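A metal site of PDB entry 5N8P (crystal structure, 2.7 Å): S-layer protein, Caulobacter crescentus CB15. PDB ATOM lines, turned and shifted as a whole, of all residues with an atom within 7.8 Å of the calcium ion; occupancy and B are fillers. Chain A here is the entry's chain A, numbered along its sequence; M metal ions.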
ATOM      1  N   SER A 253      18.155  14.464   3.666  1.00  0.00           N
ATOM      2  CA  SER A 253      17.823  13.052   3.733  1.00  0.00           C
ATOM      3  C   SER A 253      17.604  12.356   2.388  1.00  0.00           C
ATOM      4  O   SER A 253      16.713  12.746   1.653  1.00  0.00           O
ATOM      5  CB  SER A 253      16.554  12.884   4.542  1.00  0.00           C
ATOM      6  OG  SER A 253      16.886  12.780   5.890  1.00  0.00           O
ATOM      7  N   LEU A 254      18.359  11.280   2.145  1.00  0.00           N
ATOM      8  CA  LEU A 254      18.138  10.424   0.979  1.00  0.00           C
ATOM      9  C   LEU A 254      16.897   9.568   1.164  1.00  0.00           C
ATOM     10  O   LEU A 254      16.552   9.253   2.287  1.00  0.00           O
ATOM     11  CB  LEU A 254      19.342   9.520   0.719  1.00  0.00           C
ATOM     12  CG  LEU A 254      20.497  10.068  -0.144  1.00  0.00           C
ATOM     13  CD1 LEU A 254      21.323  11.068   0.618  1.00  0.00           C
ATOM     14  CD2 LEU A 254      21.395   8.933  -0.603  1.00  0.00           C
ATOM     15  N   THR A 255      16.216   9.210   0.068  1.00  0.00           N
ATOM     16  CA  THR A 255      15.019   8.345   0.071  1.00  0.00           C
ATOM     17  C   THR A 255      15.256   7.039  -0.653  1.00  0.00           C
ATOM     18  O   THR A 255      16.304   6.875  -1.265  1.00  0.00           O
ATOM     19  CB  THR A 255      13.828   9.003  -0.621  1.00  0.00           C
ATOM     20  OG1 THR A 255      14.014   8.889  -2.040  1.00  0.00           O
ATOM     21  CG2 THR A 255      13.708  10.481  -0.201  1.00  0.00           C
ATOM     22  N   THR A 256      14.300   6.125  -0.650  1.00  0.00           N
ATOM     23  CA  THR A 256      14.506   4.869  -1.393  1.00  0.00           C
ATOM     24  C   THR A 256      14.446   5.104  -2.921  1.00  0.00           C
ATOM     25  O   THR A 256      14.571   4.138  -3.690  1.00  0.00           O
ATOM     26  CB  THR A 256      13.494   3.763  -1.028  1.00  0.00           C
ATOM     27  OG1 THR A 256      12.189   4.199  -1.356  1.00  0.00           O
ATOM     28  CG2 THR A 256      13.492   3.497   0.452  1.00  0.00           C
ATOM     29  N   GLY A 257      14.304   6.355  -3.351  1.00  0.00           N
ATOM     30  CA  GLY A 257      14.308   6.711  -4.781  1.00  0.00           C
ATOM     31  C   GLY A 257      15.631   7.159  -5.441  1.00  0.00           C
ATOM     32  O   GLY A 257      16.709   6.741  -5.044  1.00  0.00           O
ATOM     33  N   THR A 258      15.528   8.002  -6.465  1.00  0.00           N
ATOM     34  CA  THR A 258      16.675   8.659  -7.017  1.00  0.00           C
ATOM     35  C   THR A 258      16.717  10.097  -6.553  1.00  0.00           C
ATOM     36  O   THR A 258      15.851  10.895  -6.877  1.00  0.00           O
ATOM     37  CB  THR A 258      16.686   8.555  -8.559  1.00  0.00           C
ATOM     38  OG1 THR A 258      16.839   7.187  -8.900  1.00  0.00           O
ATOM     39  CG2 THR A 258      17.841   9.342  -9.141  1.00  0.00           C
ATOM     40  N   ASP A 259      17.767  10.419  -5.782  1.00  0.00           N
ATOM     41  CA  ASP A 259      17.855  11.727  -5.160  1.00  0.00           C
ATOM     42  C   ASP A 259      18.834  12.603  -5.885  1.00  0.00           C
ATOM     43  O   ASP A 259      19.890  12.159  -6.327  1.00  0.00           O
ATOM     44  CB  ASP A 259      18.242  11.552  -3.704  1.00  0.00           C
ATOM     45  CG  ASP A 259      17.314  10.576  -2.971  1.00  0.00           C
ATOM     46  OD1 ASP A 259      16.133  10.940  -2.684  1.00  0.00           O
ATOM     47  OD2 ASP A 259      17.728   9.427  -2.741  1.00  0.00           O
ATOM     48  N   THR A 260      18.485  13.882  -5.997  1.00  0.00           N
ATOM     49  CA  THR A 260      19.369  14.888  -6.557  1.00  0.00           C
ATOM     50  C   THR A 260      19.525  16.015  -5.528  1.00  0.00           C
ATOM     51  O   THR A 260      18.761  16.982  -5.495  1.00  0.00           O
ATOM     52  CB  THR A 260      18.903  15.362  -7.949  1.00  0.00           C
ATOM     53  OG1 THR A 260      18.627  14.204  -8.763  1.00  0.00           O
ATOM     54  CG2 THR A 260      19.984  16.208  -8.638  1.00  0.00           C
ATOM     55  N   LEU A 261      20.539  15.885  -4.677  1.00  0.00           N
ATOM     56  CA  LEU A 261      20.680  16.731  -3.509  1.00  0.00           C
ATOM     57  C   LEU A 261      21.893  17.627  -3.622  1.00  0.00           C
ATOM     58  O   LEU A 261      22.970  17.183  -4.026  1.00  0.00           O
ATOM     59  CB  LEU A 261      20.723  15.887  -2.243  1.00  0.00           C
ATOM     60  CG  LEU A 261      19.537  14.971  -1.960  1.00  0.00           C
ATOM     61  CD1 LEU A 261      19.709  14.167  -0.679  1.00  0.00           C
ATOM     62  CD2 LEU A 261      18.182  15.716  -1.975  1.00  0.00           C
ATOM     63  N   ALA A 272      22.127   9.006   4.633  1.00  0.00           N
ATOM     64  CA  ALA A 272      21.768   7.908   3.772  1.00  0.00           C
ATOM     65  C   ALA A 272      21.444   6.663   4.580  1.00  0.00           C
ATOM     66  O   ALA A 272      22.042   5.606   4.403  1.00  0.00           O
ATOM     67  CB  ALA A 272      22.852   7.646   2.778  1.00  0.00           C
ATOM     68  N   ALA A 279      17.393   0.396   2.142  1.00  0.00           N
ATOM     69  CA  ALA A 279      18.531   1.292   1.901  1.00  0.00           C
ATOM     70  C   ALA A 279      18.138   2.593   1.200  1.00  0.00           C
ATOM     71  O   ALA A 279      17.225   2.553   0.355  1.00  0.00           O
ATOM     72  CB  ALA A 279      19.563   0.569   1.078  1.00  0.00           C
ATOM     73  N   THR A 280      18.767   3.714   1.541  1.00  0.00           N
ATOM     74  CA  THR A 280      18.464   4.966   0.806  1.00  0.00           C
ATOM     75  C   THR A 280      19.546   5.484  -0.144  1.00  0.00           C
ATOM     76  O   THR A 280      19.312   6.436  -0.902  1.00  0.00           O
ATOM     77  CB  THR A 280      17.932   6.120   1.682  1.00  0.00           C
ATOM     78  OG1 THR A 280      18.983   6.651   2.504  1.00  0.00           O
ATOM     79  CG2 THR A 280      16.765   5.672   2.516  1.00  0.00           C
ATOM     80  N   LEU A 281      20.730   4.888  -0.112  1.00  0.00           N
ATOM     81  CA  LEU A 281      21.688   5.116  -1.189  1.00  0.00           C
ATOM     82  C   LEU A 281      21.402   4.069  -2.253  1.00  0.00           C
ATOM     83  O   LEU A 281      21.585   2.869  -2.034  1.00  0.00           O
ATOM     84  CB  LEU A 281      23.128   5.120  -0.714  1.00  0.00           C
ATOM     85  CG  LEU A 281      24.130   5.768  -1.651  1.00  0.00           C
ATOM     86  CD1 LEU A 281      24.241   7.268  -1.460  1.00  0.00           C
ATOM     87  CD2 LEU A 281      25.493   5.162  -1.406  1.00  0.00           C
ATOM     88  N   THR A 282      20.896   4.542  -3.382  1.00  0.00           N
ATOM     89  CA  THR A 282      20.289   3.693  -4.423  1.00  0.00           C
ATOM     90  C   THR A 282      20.624   4.220  -5.795  1.00  0.00           C
ATOM     91  O   THR A 282      21.174   5.333  -5.932  1.00  0.00           O
ATOM     92  CB  THR A 282      18.771   3.737  -4.324  1.00  0.00           C
ATOM     93  OG1 THR A 282      18.386   5.084  -4.044  1.00  0.00           O
ATOM     94  CG2 THR A 282      18.258   2.830  -3.197  1.00  0.00           C
ATOM     95  N   VAL A 283      20.247   3.462  -6.824  1.00  0.00           N
ATOM     96  CA  VAL A 283      20.613   3.779  -8.198  1.00  0.00           C
ATOM     97  C   VAL A 283      20.341   5.230  -8.612  1.00  0.00           C
ATOM     98  O   VAL A 283      19.288   5.754  -8.349  1.00  0.00           O
ATOM     99  CB  VAL A 283      20.147   2.681  -9.225  1.00  0.00           C
ATOM    100  CG1 VAL A 283      19.778   1.347  -8.555  1.00  0.00           C
ATOM    101  CG2 VAL A 283      18.917   3.089  -9.936  1.00  0.00           C
ATOM    102  N   GLY A 284      21.356   5.876  -9.199  1.00  0.00           N
ATOM    103  CA  GLY A 284      21.248   7.218  -9.771  1.00  0.00           C
ATOM    104  C   GLY A 284      21.381   8.375  -8.801  1.00  0.00           C
ATOM    105  O   GLY A 284      21.459   9.537  -9.260  1.00  0.00           O
ATOM    106  N   ASP A 285      21.383   8.090  -7.501  1.00  0.00           N
ATOM    107  CA  ASP A 285      21.558   9.106  -6.473  1.00  0.00           C
ATOM    108  C   ASP A 285      22.743  10.022  -6.796  1.00  0.00           C
ATOM    109  O   ASP A 285      23.870   9.547  -6.951  1.00  0.00           O
ATOM    110  CB  ASP A 285      21.784   8.472  -5.093  1.00  0.00           C
ATOM    111  CG  ASP A 285      20.521   7.934  -4.436  1.00  0.00           C
ATOM    112  OD1 ASP A 285      20.652   7.181  -3.443  1.00  0.00           O
ATOM    113  OD2 ASP A 285      19.382   8.251  -4.861  1.00  0.00           O
ATOM    114  N   THR A 286      22.513  11.322  -6.912  1.00  0.00           N
ATOM    115  CA  THR A 286      23.664  12.217  -7.073  1.00  0.00           C
ATOM    116  C   THR A 286      23.670  13.303  -6.009  1.00  0.00           C
ATOM    117  O   THR A 286      22.684  14.028  -5.818  1.00  0.00           O
ATOM    118  CB  THR A 286      23.855  12.763  -8.530  1.00  0.00           C
ATOM    119  OG1 THR A 286      22.880  13.761  -8.799  1.00  0.00           O
ATOM    120  CG2 THR A 286      23.807  11.657  -9.643  1.00  0.00           C
ATOM    121  N   LEU A 287      24.808  13.385  -5.302  1.00  0.00           N
ATOM    122  CA  LEU A 287      24.978  14.301  -4.164  1.00  0.00           C
ATOM    123  C   LEU A 287      26.085  15.306  -4.413  1.00  0.00           C
ATOM    124  O   LEU A 287      27.126  14.963  -4.965  1.00  0.00           O
ATOM    125  CB  LEU A 287      25.192  13.527  -2.854  1.00  0.00           C
ATOM    126  CG  LEU A 287      24.337  12.302  -2.576  1.00  0.00           C
ATOM    127  CD1 LEU A 287      24.944  11.430  -1.481  1.00  0.00           C
ATOM    128  CD2 LEU A 287      22.895  12.726  -2.298  1.00  0.00           C
ATOM    129  N   VAL A 311      25.451   6.302  -9.096  1.00  0.00           N
ATOM    130  CA  VAL A 311      25.724   7.098  -7.902  1.00  0.00           C
ATOM    131  C   VAL A 311      26.984   7.924  -8.118  1.00  0.00           C
ATOM    132  O   VAL A 311      27.988   7.390  -8.589  1.00  0.00           O
ATOM    133  CB  VAL A 311      25.798   6.234  -6.618  1.00  0.00           C
ATOM    134  CG1 VAL A 311      26.331   7.041  -5.414  1.00  0.00           C
ATOM    135  CG2 VAL A 311      24.432   5.677  -6.267  1.00  0.00           C
HETATM  136 CA    CA M   1      18.213   7.179  -2.859  1.00  0.00          CA
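The nearest printed residue that does not touch the calcium ion is Leu 254 (4.3 Å).
The backbone NH (N) of Thr 286 sits at hydrogen-bond distance from the backbone carbonyl oxygen (O) of Asp 259, at 2.8 Å. The side-chain hydroxyl (OG1) of Thr 255 is in hydrogen-bond range of the backbone NH (N) of Gly 257 (2.9 Å).
The calcium ion is bound by OD2 of Asp 259 (2.3 Å). O of Thr 280 is bound to the calcium ion (2.4 Å). The calcium ion is bound by OG1 of Thr 282, at 2.4 Å. O of Thr 255 binds the calcium ion (2.5 Å). The calcium ion is bound by OD1 of Asp 285, at 2.5 Å. OD2 of Asp 285 is bound to the calcium ion, at 2.6 Å. The backbone carbonyl oxygen (O) of Gly 257 binds the calcium ion, at 2.7 Å.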
